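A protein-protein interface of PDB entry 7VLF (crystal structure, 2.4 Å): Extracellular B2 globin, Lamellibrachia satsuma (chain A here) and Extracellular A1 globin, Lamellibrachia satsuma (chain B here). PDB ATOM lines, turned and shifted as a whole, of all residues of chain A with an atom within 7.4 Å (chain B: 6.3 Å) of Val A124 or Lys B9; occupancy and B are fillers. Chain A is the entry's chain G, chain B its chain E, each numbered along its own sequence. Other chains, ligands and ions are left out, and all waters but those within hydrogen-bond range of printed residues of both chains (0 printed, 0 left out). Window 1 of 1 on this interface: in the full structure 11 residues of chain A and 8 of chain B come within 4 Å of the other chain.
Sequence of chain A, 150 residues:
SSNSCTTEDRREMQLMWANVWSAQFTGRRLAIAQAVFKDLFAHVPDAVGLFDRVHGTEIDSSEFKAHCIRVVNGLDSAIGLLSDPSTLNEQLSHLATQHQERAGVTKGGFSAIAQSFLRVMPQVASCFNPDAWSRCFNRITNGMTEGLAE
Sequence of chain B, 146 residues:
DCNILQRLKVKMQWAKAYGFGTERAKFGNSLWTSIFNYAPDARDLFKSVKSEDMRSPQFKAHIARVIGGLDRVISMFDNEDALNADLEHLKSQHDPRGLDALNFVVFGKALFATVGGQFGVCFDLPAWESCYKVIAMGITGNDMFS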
ATOM      1  N   MET A  16     -24.133 -10.220 -13.607  1.00  0.00           N
ATOM      2  CA  MET A  16     -23.772  -8.895 -14.099  1.00  0.00           C
ATOM      3  C   MET A  16     -24.908  -8.270 -14.895  1.00  0.00           C
ATOM      4  O   MET A  16     -25.201  -7.078 -14.742  1.00  0.00           O
ATOM      5  CB  MET A  16     -22.516  -8.984 -14.959  1.00  0.00           C
ATOM      6  CG  MET A  16     -22.144  -7.683 -15.621  1.00  0.00           C
ATOM      7  SD  MET A  16     -21.684  -7.926 -17.341  1.00  0.00           S
ATOM      8  CE  MET A  16     -23.279  -8.283 -18.069  1.00  0.00           C
ATOM      9  N   ASN A  19     -28.247  -6.831 -12.912  1.00  0.00           N
ATOM     10  CA  ASN A  19     -28.238  -5.515 -12.289  1.00  0.00           C
ATOM     11  C   ASN A  19     -28.343  -4.402 -13.326  1.00  0.00           C
ATOM     12  O   ASN A  19     -29.020  -3.394 -13.091  1.00  0.00           O
ATOM     13  CB  ASN A  19     -26.977  -5.342 -11.447  1.00  0.00           C
ATOM     14  CG  ASN A  19     -27.274  -5.305  -9.965  1.00  0.00           C
ATOM     15  OD1 ASN A  19     -28.339  -5.736  -9.522  1.00  0.00           O
ATOM     16  ND2 ASN A  19     -26.334  -4.781  -9.186  1.00  0.00           N
ATOM     17  N   VAL A  20     -27.691  -4.572 -14.480  1.00  0.00           N
ATOM     18  CA  VAL A  20     -27.656  -3.505 -15.474  1.00  0.00           C
ATOM     19  C   VAL A  20     -28.903  -3.482 -16.349  1.00  0.00           C
ATOM     20  O   VAL A  20     -29.174  -2.465 -16.996  1.00  0.00           O
ATOM     21  CB  VAL A  20     -26.401  -3.634 -16.348  1.00  0.00           C
ATOM     22  CG1 VAL A  20     -25.189  -3.866 -15.468  1.00  0.00           C
ATOM     23  CG2 VAL A  20     -26.567  -4.756 -17.353  1.00  0.00           C
ATOM     24  N   TRP A  21     -29.672  -4.564 -16.388  1.00  0.00           N
ATOM     25  CA  TRP A  21     -30.939  -4.604 -17.107  1.00  0.00           C
ATOM     26  C   TRP A  21     -32.034  -5.011 -16.136  1.00  0.00           C
ATOM     27  O   TRP A  21     -31.852  -5.949 -15.352  1.00  0.00           O
ATOM     28  CB  TRP A  21     -30.879  -5.576 -18.284  1.00  0.00           C
ATOM     29  CG  TRP A  21     -32.198  -5.821 -18.949  1.00  0.00           C
ATOM     30  CD1 TRP A  21     -33.196  -6.649 -18.521  1.00  0.00           C
ATOM     31  CD2 TRP A  21     -32.654  -5.252 -20.181  1.00  0.00           C
ATOM     32  NE1 TRP A  21     -34.247  -6.623 -19.402  1.00  0.00           N
ATOM     33  CE2 TRP A  21     -33.939  -5.773 -20.431  1.00  0.00           C
ATOM     34  CE3 TRP A  21     -32.103  -4.349 -21.097  1.00  0.00           C
ATOM     35  CZ2 TRP A  21     -34.680  -5.424 -21.557  1.00  0.00           C
ATOM     36  CZ3 TRP A  21     -32.843  -4.002 -22.210  1.00  0.00           C
ATOM     37  CH2 TRP A  21     -34.116  -4.538 -22.431  1.00  0.00           C
ATOM     38  N   ARG A  28     -32.600   3.024 -18.280  1.00  0.00           N
ATOM     39  CA  ARG A  28     -31.331   2.309 -18.366  1.00  0.00           C
ATOM     40  C   ARG A  28     -31.336   1.309 -19.513  1.00  0.00           C
ATOM     41  O   ARG A  28     -30.298   1.086 -20.147  1.00  0.00           O
ATOM     42  CB  ARG A  28     -31.014   1.601 -17.046  1.00  0.00           C
ATOM     43  CG  ARG A  28     -29.647   0.927 -17.059  1.00  0.00           C
ATOM     44  CD  ARG A  28     -29.209   0.465 -15.680  1.00  0.00           C
ATOM     45  NE  ARG A  28     -29.634   1.389 -14.633  1.00  0.00           N
ATOM     46  CZ  ARG A  28     -30.146   1.002 -13.470  1.00  0.00           C
ATOM     47  NH1 ARG A  28     -30.514   1.901 -12.568  1.00  0.00           N
ATOM     48  NH2 ARG A  28     -30.290  -0.290 -13.207  1.00  0.00           N
ATOM     49  N   ALA A  31     -30.677   3.317 -23.029  1.00  0.00           N
ATOM     50  CA  ALA A  31     -29.327   3.817 -23.268  1.00  0.00           C
ATOM     51  C   ALA A  31     -28.403   2.701 -23.732  1.00  0.00           C
ATOM     52  O   ALA A  31     -27.622   2.880 -24.673  1.00  0.00           O
ATOM     53  CB  ALA A  31     -28.780   4.480 -22.007  1.00  0.00           C
ATOM     54  N   ILE A  32     -28.475   1.540 -23.078  1.00  0.00           N
ATOM     55  CA  ILE A  32     -27.702   0.386 -23.529  1.00  0.00           C
ATOM     56  C   ILE A  32     -28.135  -0.020 -24.932  1.00  0.00           C
ATOM     57  O   ILE A  32     -27.308  -0.402 -25.771  1.00  0.00           O
ATOM     58  CB  ILE A  32     -27.850  -0.782 -22.537  1.00  0.00           C
ATOM     59  CG1 ILE A  32     -27.569  -0.321 -21.107  1.00  0.00           C
ATOM     60  CG2 ILE A  32     -26.916  -1.918 -22.912  1.00  0.00           C
ATOM     61  CD1 ILE A  32     -27.840  -1.388 -20.066  1.00  0.00           C
ATOM     62  N   ARG A 119     -17.818  -3.577 -26.420  1.00  0.00           N
ATOM     63  CA  ARG A 119     -17.415  -2.195 -26.192  1.00  0.00           C
ATOM     64  C   ARG A 119     -18.376  -1.437 -25.285  1.00  0.00           C
ATOM     65  O   ARG A 119     -17.937  -0.615 -24.474  1.00  0.00           O
ATOM     66  CB  ARG A 119     -17.298  -1.447 -27.525  1.00  0.00           C
ATOM     67  CG  ARG A 119     -16.314  -2.047 -28.521  1.00  0.00           C
ATOM     68  CD  ARG A 119     -16.322  -1.254 -29.825  1.00  0.00           C
ATOM     69  NE  ARG A 119     -15.702  -1.971 -30.938  1.00  0.00           N
ATOM     70  CZ  ARG A 119     -16.365  -2.424 -32.000  1.00  0.00           C
ATOM     71  NH1 ARG A 119     -15.719  -3.061 -32.969  1.00  0.00           N
ATOM     72  NH2 ARG A 119     -17.672  -2.227 -32.100  1.00  0.00           N
ATOM     73  N   VAL A 120     -19.678  -1.693 -25.405  1.00  0.00           N
ATOM     74  CA  VAL A 120     -20.666  -0.901 -24.680  1.00  0.00           C
ATOM     75  C   VAL A 120     -20.839  -1.408 -23.253  1.00  0.00           C
ATOM     76  O   VAL A 120     -20.947  -0.616 -22.312  1.00  0.00           O
ATOM     77  CB  VAL A 120     -21.999  -0.900 -25.447  1.00  0.00           C
ATOM     78  CG1 VAL A 120     -23.100  -0.283 -24.600  1.00  0.00           C
ATOM     79  CG2 VAL A 120     -21.847  -0.149 -26.760  1.00  0.00           C
ATOM     80  N   MET A 121     -20.861  -2.729 -23.071  1.00  0.00           N
ATOM     81  CA  MET A 121     -21.181  -3.300 -21.763  1.00  0.00           C
ATOM     82  C   MET A 121     -20.204  -2.909 -20.659  1.00  0.00           C
ATOM     83  O   MET A 121     -20.668  -2.543 -19.565  1.00  0.00           O
ATOM     84  CB  MET A 121     -21.291  -4.823 -21.887  1.00  0.00           C
ATOM     85  CG  MET A 121     -22.487  -5.294 -22.703  1.00  0.00           C
ATOM     86  SD  MET A 121     -24.058  -4.693 -22.049  1.00  0.00           S
ATOM     87  CE  MET A 121     -24.062  -5.434 -20.420  1.00  0.00           C
ATOM     88  N   PRO A 122     -18.877  -2.960 -20.845  1.00  0.00           N
ATOM     89  CA  PRO A 122     -17.979  -2.654 -19.717  1.00  0.00           C
ATOM     90  C   PRO A 122     -18.114  -1.239 -19.194  1.00  0.00           C
ATOM     91  O   PRO A 122     -17.643  -0.959 -18.087  1.00  0.00           O
ATOM     92  CB  PRO A 122     -16.582  -2.898 -20.301  1.00  0.00           C
ATOM     93  CG  PRO A 122     -16.757  -2.759 -21.769  1.00  0.00           C
ATOM     94  CD  PRO A 122     -18.112  -3.316 -22.054  1.00  0.00           C
ATOM     95  N   GLN A 123     -18.744  -0.340 -19.939  1.00  0.00           N
ATOM     96  CA  GLN A 123     -18.892   1.031 -19.484  1.00  0.00           C
ATOM     97  C   GLN A 123     -20.142   1.237 -18.636  1.00  0.00           C
ATOM     98  O   GLN A 123     -20.217   2.212 -17.880  1.00  0.00           O
ATOM     99  CB  GLN A 123     -18.933   1.971 -20.687  1.00  0.00           C
ATOM    100  CG  GLN A 123     -17.973   1.567 -21.809  1.00  0.00           C
ATOM    101  CD  GLN A 123     -18.174   2.375 -23.080  1.00  0.00           C
ATOM    102  OE1 GLN A 123     -18.529   3.549 -23.028  1.00  0.00           O
ATOM    103  NE2 GLN A 123     -17.955   1.741 -24.231  1.00  0.00           N
ATOM    104  N   VAL A 124     -21.155   0.401 -18.797  1.00  0.00           N
ATOM    105  CA  VAL A 124     -22.347   0.512 -17.976  1.00  0.00           C
ATOM    106  C   VAL A 124     -22.414  -0.589 -16.929  1.00  0.00           C
ATOM    107  O   VAL A 124     -22.926  -0.352 -15.826  1.00  0.00           O
ATOM    108  CB  VAL A 124     -23.619   0.515 -18.858  1.00  0.00           C
ATOM    109  CG1 VAL A 124     -23.685  -0.716 -19.740  1.00  0.00           C
ATOM    110  CG2 VAL A 124     -24.888   0.618 -18.002  1.00  0.00           C
ATOM    111  N   ALA A 125     -21.896  -1.783 -17.249  1.00  0.00           N
ATOM    112  CA  ALA A 125     -21.885  -2.937 -16.361  1.00  0.00           C
ATOM    113  C   ALA A 125     -20.591  -2.952 -15.560  1.00  0.00           C
ATOM    114  O   ALA A 125     -19.491  -2.882 -16.122  1.00  0.00           O
ATOM    115  CB  ALA A 125     -22.032  -4.241 -17.150  1.00  0.00           C
ATOM    116  N   SER A 126     -20.738  -3.009 -14.250  1.00  0.00           N
ATOM    117  CA  SER A 126     -19.615  -3.221 -13.356  1.00  0.00           C
ATOM    118  C   SER A 126     -19.259  -4.701 -13.299  1.00  0.00           C
ATOM    119  O   SER A 126     -20.107  -5.574 -13.506  1.00  0.00           O
ATOM    120  CB  SER A 126     -19.951  -2.709 -11.955  1.00  0.00           C
ATOM    121  OG  SER A 126     -20.223  -1.315 -11.978  1.00  0.00           O
ATOM    122  N   CYS A 127     -17.987  -4.971 -12.997  1.00  0.00           N
ATOM    123  CA  CYS A 127     -17.430  -6.321 -12.983  1.00  0.00           C
ATOM    124  C   CYS A 127     -17.644  -7.036 -14.312  1.00  0.00           C
ATOM    125  O   CYS A 127     -17.813  -8.256 -14.343  1.00  0.00           O
ATOM    126  CB  CYS A 127     -18.014  -7.163 -11.843  1.00  0.00           C
ATOM    127  SG  CYS A 127     -18.371  -6.336 -10.275  1.00  0.00           S
ATOM    128  N   PHE A 128     -17.633  -6.298 -15.421  1.00  0.00           N
ATOM    129  CA  PHE A 128     -17.863  -6.919 -16.717  1.00  0.00           C
ATOM    130  C   PHE A 128     -16.724  -7.866 -17.070  1.00  0.00           C
ATOM    131  O   PHE A 128     -15.546  -7.545 -16.890  1.00  0.00           O
ATOM    132  CB  PHE A 128     -18.018  -5.859 -17.808  1.00  0.00           C
ATOM    133  CG  PHE A 128     -18.153  -6.434 -19.193  1.00  0.00           C
ATOM    134  CD1 PHE A 128     -19.336  -7.026 -19.600  1.00  0.00           C
ATOM    135  CD2 PHE A 128     -17.094  -6.388 -20.084  1.00  0.00           C
ATOM    136  CE1 PHE A 128     -19.461  -7.561 -20.869  1.00  0.00           C
ATOM    137  CE2 PHE A 128     -17.214  -6.919 -21.357  1.00  0.00           C
ATOM    138  CZ  PHE A 128     -18.400  -7.506 -21.748  1.00  0.00           C
ATOM    139  N   ILE B   4     -23.692   9.028 -21.336  1.00  0.00           N
ATOM    140  CA  ILE B   4     -24.858   8.504 -20.633  1.00  0.00           C
ATOM    141  C   ILE B   4     -24.581   7.113 -20.073  1.00  0.00           C
ATOM    142  O   ILE B   4     -25.101   6.749 -19.009  1.00  0.00           O
ATOM    143  CB  ILE B   4     -26.081   8.512 -21.569  1.00  0.00           C
ATOM    144  CG1 ILE B   4     -27.275   7.827 -20.905  1.00  0.00           C
ATOM    145  CG2 ILE B   4     -25.748   7.846 -22.888  1.00  0.00           C
ATOM    146  CD1 ILE B   4     -27.769   8.533 -19.674  1.00  0.00           C
ATOM    147  N   LEU B   5     -23.750   6.322 -20.758  1.00  0.00           N
ATOM    148  CA  LEU B   5     -23.364   5.021 -20.221  1.00  0.00           C
ATOM    149  C   LEU B   5     -22.634   5.176 -18.894  1.00  0.00           C
ATOM    150  O   LEU B   5     -22.954   4.496 -17.912  1.00  0.00           O
ATOM    151  CB  LEU B   5     -22.493   4.273 -21.231  1.00  0.00           C
ATOM    152  CG  LEU B   5     -23.118   3.908 -22.577  1.00  0.00           C
ATOM    153  CD1 LEU B   5     -22.091   3.220 -23.461  1.00  0.00           C
ATOM    154  CD2 LEU B   5     -24.341   3.025 -22.383  1.00  0.00           C
ATOM    155  N   GLN B   6     -21.645   6.073 -18.848  1.00  0.00           N
ATOM    156  CA  GLN B   6     -20.965   6.354 -17.590  1.00  0.00           C
ATOM    157  C   GLN B   6     -21.909   6.983 -16.575  1.00  0.00           C
ATOM    158  O   GLN B   6     -21.754   6.767 -15.368  1.00  0.00           O
ATOM    159  CB  GLN B   6     -19.762   7.267 -17.832  1.00  0.00           C
ATOM    160  CG  GLN B   6     -18.671   6.644 -18.689  1.00  0.00           C
ATOM    161  CD  GLN B   6     -17.525   7.599 -18.958  1.00  0.00           C
ATOM    162  OE1 GLN B   6     -17.684   8.816 -18.872  1.00  0.00           O
ATOM    163  NE2 GLN B   6     -16.358   7.051 -19.284  1.00  0.00           N
ATOM    164  N   ARG B   7     -22.893   7.756 -17.042  1.00  0.00           N
ATOM    165  CA  ARG B   7     -23.863   8.352 -16.129  1.00  0.00           C
ATOM    166  C   ARG B   7     -24.705   7.285 -15.441  1.00  0.00           C
ATOM    167  O   ARG B   7     -25.026   7.407 -14.254  1.00  0.00           O
ATOM    168  CB  ARG B   7     -24.759   9.337 -16.883  1.00  0.00           C
ATOM    169  CG  ARG B   7     -24.019  10.538 -17.432  1.00  0.00           C
ATOM    170  CD  ARG B   7     -24.900  11.382 -18.333  1.00  0.00           C
ATOM    171  NE  ARG B   7     -24.166  12.500 -18.919  1.00  0.00           N
ATOM    172  CZ  ARG B   7     -24.081  13.709 -18.373  1.00  0.00           C
ATOM    173  NH1 ARG B   7     -24.690  13.962 -17.223  1.00  0.00           N
ATOM    174  NH2 ARG B   7     -23.391  14.667 -18.975  1.00  0.00           N
ATOM    175  N   LEU B   8     -25.062   6.224 -16.167  1.00  0.00           N
ATOM    176  CA  LEU B   8     -25.929   5.198 -15.597  1.00  0.00           C
ATOM    177  C   LEU B   8     -25.168   4.282 -14.648  1.00  0.00           C
ATOM    178  O   LEU B   8     -25.722   3.837 -13.636  1.00  0.00           O
ATOM    179  CB  LEU B   8     -26.587   4.388 -16.715  1.00  0.00           C
ATOM    180  CG  LEU B   8     -27.648   5.136 -17.527  1.00  0.00           C
ATOM    181  CD1 LEU B   8     -28.308   4.201 -18.518  1.00  0.00           C
ATOM    182  CD2 LEU B   8     -28.686   5.771 -16.613  1.00  0.00           C
ATOM    183  N   LYS B   9     -23.905   3.984 -14.955  1.00  0.00           N
ATOM    184  CA  LYS B   9     -23.145   3.110 -14.069  1.00  0.00           C
ATOM    185  C   LYS B   9     -22.834   3.807 -12.749  1.00  0.00           C
ATOM    186  O   LYS B   9     -22.866   3.173 -11.689  1.00  0.00           O
ATOM    187  CB  LYS B   9     -21.861   2.634 -14.745  1.00  0.00           C
ATOM    188  CG  LYS B   9     -21.086   1.653 -13.893  1.00  0.00           C
ATOM    189  CD  LYS B   9     -19.613   1.674 -14.240  1.00  0.00           C
ATOM    190  CE  LYS B   9     -19.284   0.547 -15.206  1.00  0.00           C
ATOM    191  NZ  LYS B   9     -17.867   0.074 -15.155  1.00  0.00           N
ATOM    192  N   VAL B  10     -22.540   5.111 -12.795  1.00  0.00           N
ATOM    193  CA  VAL B  10     -22.308   5.869 -11.567  1.00  0.00           C
ATOM    194  C   VAL B  10     -23.511   5.766 -10.637  1.00  0.00           C
ATOM    195  O   VAL B  10     -23.361   5.532  -9.432  1.00  0.00           O
ATOM    196  CB  VAL B  10     -21.963   7.335 -11.895  1.00  0.00           C
ATOM    197  CG1 VAL B  10     -22.060   8.204 -10.652  1.00  0.00           C
ATOM    198  CG2 VAL B  10     -20.567   7.427 -12.490  1.00  0.00           C
ATOM    199  N   LYS B  11     -24.719   5.922 -11.183  1.00  0.00           N
ATOM    200  CA  LYS B  11     -25.929   5.792 -10.374  1.00  0.00           C
ATOM    201  C   LYS B  11     -26.016   4.416  -9.726  1.00  0.00           C
ATOM    202  O   LYS B  11     -26.296   4.298  -8.526  1.00  0.00           O
ATOM    203  CB  LYS B  11     -27.163   6.060 -11.235  1.00  0.00           C
ATOM    204  CG  LYS B  11     -28.464   5.568 -10.632  1.00  0.00           C
ATOM    205  CD  LYS B  11     -29.610   5.775 -11.601  1.00  0.00           C
ATOM    206  CE  LYS B  11     -29.751   7.245 -11.956  1.00  0.00           C
ATOM    207  NZ  LYS B  11     -30.888   7.501 -12.882  1.00  0.00           N
ATOM    208  N   MET B  12     -25.764   3.359 -10.500  1.00  0.00           N
ATOM    209  CA  MET B  12     -25.814   2.011  -9.940  1.00  0.00           C
ATOM    210  C   MET B  12     -24.733   1.820  -8.883  1.00  0.00           C
ATOM    211  O   MET B  12     -24.984   1.249  -7.816  1.00  0.00           O
ATOM    212  CB  MET B  12     -25.670   0.967 -11.048  1.00  0.00           C
ATOM    213  CG  MET B  12     -26.813   0.959 -12.039  1.00  0.00           C
ATOM    214  SD  MET B  12     -27.399  -0.708 -12.386  1.00  0.00           S
ATOM    215  CE  MET B  12     -28.071  -1.172 -10.789  1.00  0.00           C
ATOM    216  N   GLN B  13     -23.516   2.288  -9.171  1.00  0.00           N
ATOM    217  CA  GLN B  13     -22.442   2.203  -8.188  1.00  0.00           C
ATOM    218  C   GLN B  13     -22.704   3.106  -6.991  1.00  0.00           C
ATOM    219  O   GLN B  13     -22.258   2.802  -5.879  1.00  0.00           O
ATOM    220  CB  GLN B  13     -21.104   2.558  -8.838  1.00  0.00           C
ATOM    221  CG  GLN B  13     -20.637   1.564  -9.888  1.00  0.00           C
ATOM    222  CD  GLN B  13     -19.180   1.759 -10.261  1.00  0.00           C
ATOM    223  OE1 GLN B  13     -18.522   2.673  -9.768  1.00  0.00           O
ATOM    224  NE2 GLN B  13     -18.668   0.894 -11.130  1.00  0.00           N
ATOM    225  N   TRP B  14     -23.425   4.211  -7.190  1.00  0.00           N
ATOM    226  CA  TRP B  14     -23.719   5.110  -6.080  1.00  0.00           C
ATOM    227  C   TRP B  14     -24.827   4.556  -5.194  1.00  0.00           C
ATOM    228  O   TRP B  14     -24.673   4.486  -3.971  1.00  0.00           O
ATOM    229  CB  TRP B  14     -24.099   6.494  -6.605  1.00  0.00           C
ATOM    230  CG  TRP B  14     -24.770   7.355  -5.588  1.00  0.00           C
ATOM    231  CD1 TRP B  14     -26.098   7.639  -5.511  1.00  0.00           C
ATOM    232  CD2 TRP B  14     -24.148   8.044  -4.499  1.00  0.00           C
ATOM    233  NE1 TRP B  14     -26.346   8.463  -4.443  1.00  0.00           N
ATOM    234  CE2 TRP B  14     -25.164   8.727  -3.804  1.00  0.00           C
ATOM    235  CE3 TRP B  14     -22.830   8.151  -4.045  1.00  0.00           C
ATOM    236  CZ2 TRP B  14     -24.906   9.506  -2.682  1.00  0.00           C
ATOM    237  CZ3 TRP B  14     -22.576   8.923  -2.930  1.00  0.00           C
ATOM    238  CH2 TRP B  14     -23.608   9.591  -2.260  1.00  0.00           C
ATOM    239  N   CYS B 122     -14.829  -3.457  -8.285  1.00  0.00           N
ATOM    240  CA  CYS B 122     -15.435  -3.094  -9.570  1.00  0.00           C
ATOM    241  C   CYS B 122     -15.734  -1.605  -9.694  1.00  0.00           C
ATOM    242  O   CYS B 122     -16.370  -1.233 -10.685  1.00  0.00           O
ATOM    243  CB  CYS B 122     -16.721  -3.883  -9.797  1.00  0.00           C
ATOM    244  SG  CYS B 122     -16.579  -5.664  -9.603  1.00  0.00           S
ATOM    245  N   PHE B 123     -15.317  -0.782  -8.733  1.00  0.00           N
ATOM    246  CA  PHE B 123     -15.543   0.655  -8.807  1.00  0.00           C
ATOM    247  C   PHE B 123     -14.895   1.233 -10.058  1.00  0.00           C
ATOM    248  O   PHE B 123     -13.708   1.016 -10.315  1.00  0.00           O
ATOM    249  CB  PHE B 123     -14.987   1.330  -7.553  1.00  0.00           C
ATOM    250  CG  PHE B 123     -15.088   2.829  -7.568  1.00  0.00           C
ATOM    251  CD1 PHE B 123     -16.313   3.455  -7.416  1.00  0.00           C
ATOM    252  CD2 PHE B 123     -13.953   3.613  -7.714  1.00  0.00           C
ATOM    253  CE1 PHE B 123     -16.406   4.836  -7.424  1.00  0.00           C
ATOM    254  CE2 PHE B 123     -14.041   4.992  -7.721  1.00  0.00           C
ATOM    255  CZ  PHE B 123     -15.268   5.603  -7.576  1.00  0.00           C
ATOM    256  N   ASP B 124     -15.686   1.966 -10.839  1.00  0.00           N
ATOM    257  CA  ASP B 124     -15.217   2.556 -12.094  1.00  0.00           C
ATOM    258  C   ASP B 124     -14.699   3.957 -11.792  1.00  0.00           C
ATOM    259  O   ASP B 124     -15.445   4.937 -11.814  1.00  0.00           O
ATOM    260  CB  ASP B 124     -16.336   2.573 -13.129  1.00  0.00           C
ATOM    261  CG  ASP B 124     -15.832   2.828 -14.539  1.00  0.00           C
ATOM    262  OD1 ASP B 124     -14.939   3.686 -14.711  1.00  0.00           O
ATOM    263  OD2 ASP B 124     -16.327   2.175 -15.479  1.00  0.00           O
ATOM    264  N   ALA B 127     -14.919   6.614 -14.901  1.00  0.00           N
ATOM    265  CA  ALA B 127     -16.268   7.123 -15.128  1.00  0.00           C
ATOM    266  C   ALA B 127     -16.678   8.102 -14.034  1.00  0.00           C
ATOM    267  O   ALA B 127     -17.277   9.147 -14.318  1.00  0.00           O
ATOM    268  CB  ALA B 127     -17.258   5.962 -15.221  1.00  0.00           C
ATOM    269  N   TRP B 128     -16.351   7.789 -12.779  1.00  0.00           N
ATOM    270  CA  TRP B 128     -16.626   8.718 -11.688  1.00  0.00           C
ATOM    271  C   TRP B 128     -15.810   9.998 -11.813  1.00  0.00           C
ATOM    272  O   TRP B 128     -16.284  11.071 -11.426  1.00  0.00           O
ATOM    273  CB  TRP B 128     -16.358   8.039 -10.347  1.00  0.00           C
ATOM    274  CG  TRP B 128     -17.493   7.198  -9.865  1.00  0.00           C
ATOM    275  CD1 TRP B 128     -17.812   5.938 -10.275  1.00  0.00           C
ATOM    276  CD2 TRP B 128     -18.466   7.555  -8.875  1.00  0.00           C
ATOM    277  NE1 TRP B 128     -18.924   5.489  -9.605  1.00  0.00           N
ATOM    278  CE2 TRP B 128     -19.345   6.464  -8.740  1.00  0.00           C
ATOM    279  CE3 TRP B 128     -18.679   8.694  -8.092  1.00  0.00           C
ATOM    280  CZ2 TRP B 128     -20.420   6.476  -7.855  1.00  0.00           C
ATOM    281  CZ3 TRP B 128     -19.748   8.704  -7.212  1.00  0.00           C
ATOM    282  CH2 TRP B 128     -20.605   7.602  -7.101  1.00  0.00           C
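The side-chain amino group (NZ) of Lys B9 is in salt-bridge range of the side-chain carboxylate (OD2) of Asp B124 (2.6 Å).
The side-chain amide oxygen of Gln B13 sits at hydrogen-bond distance from the indole nitrogen of Trp B128, 2.8 Å away.
NE2 of Gln B13 lies within hydrogen-bond range of O of Cys B122 (3.2 Å).
The backbone NH (N) of Asp B124 is in hydrogen-bond range of the side-chain amide oxygen (OE1) of Gln B13 (3.1 Å).
NH2 of Arg A28 is in hydrogen-bond range of O of Asn A19 (3.4 Å).
Of the 16 printed residues of chain B, 7 touch a printed residue of chain A.
Hydrophobic or aromatic side chains of chain B that line the printed part of chain A: Ile B4, Leu B5, Leu B8 and Met B12.
Of the 17 printed residues of chain A, 10 touch a printed residue of chain B.
Among the printed residues, 14 pairs touch across the chains.
The side-chain amide nitrogen (NE2) of Gln B13 lies within hydrogen-bond range of the side-chain hydroxyl (OG) of Ser A126 (2.8 Å).
The side-chain sulfur (SD) of Met B12 is in hydrogen-bond range of the guanidinium group (NH2) of Arg A28, at 3.0 Å.
The side-chain amino group (NZ) of Lys B9 sits at hydrogen-bond distance from the backbone carbonyl oxygen (O) of Pro A122 (3.1 Å).
The backbone carbonyl oxygen of Asn A19 lies close to the side-chain sulfur of Met B12 (3.2 Å).
The side-chain sulfur (SG) of Cys B122 forms a disulfide with the side-chain sulfur (SG) of Cys A127 (2.0 Å).
Of the printed residues of chain B, Ala A31 touches Ile B4 (3.8 Å) and Leu B8 (3.5 Å).
Arg A119 touches none of the printed residues of chain B.
Val A124 touches just one residue of chain B: Lys B9 (3.3 Å).
Of the printed residues of chain B, Ala A125 touches Lys B9 (3.5 Å).
Of chain A, only Pro A122 (3.1 Å), Gln A123 (3.3 Å), Val A124 (3.3 Å), Ala A125 (3.5 Å) and Ser A126 (3.6 Å) come within 4 Å of Lys B9.
The nearest residue of chain A that does not touch Lys B9 is Cys A127 (5.5 Å).
The nearest printed residue of chain B that does not touch Arg A28 is Lys B11 (4.1 Å).
Arg A28 touches Leu B8.
CG1 of Ile B4 touches CB of Ala A31, 3.8 Å away.
Ala A31 touches Leu B8 (CB to CD1, 3.5 Å).
Leu B5 touches Val A120 (CD1 to CG1, 3.8 Å).
Gln A123 touches Leu B5 (O to O, 3.6 Å).
CE of Lys B9 touches O of Gln A123, 3.3 Å away.
CG of Lys B9 touches O of Val A124, at 3.3 Å.
NZ of Lys B9 touches O of Ala A125, at 3.5 Å.
OG of Ser A126 touches CG of Lys B9, 3.6 Å away.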
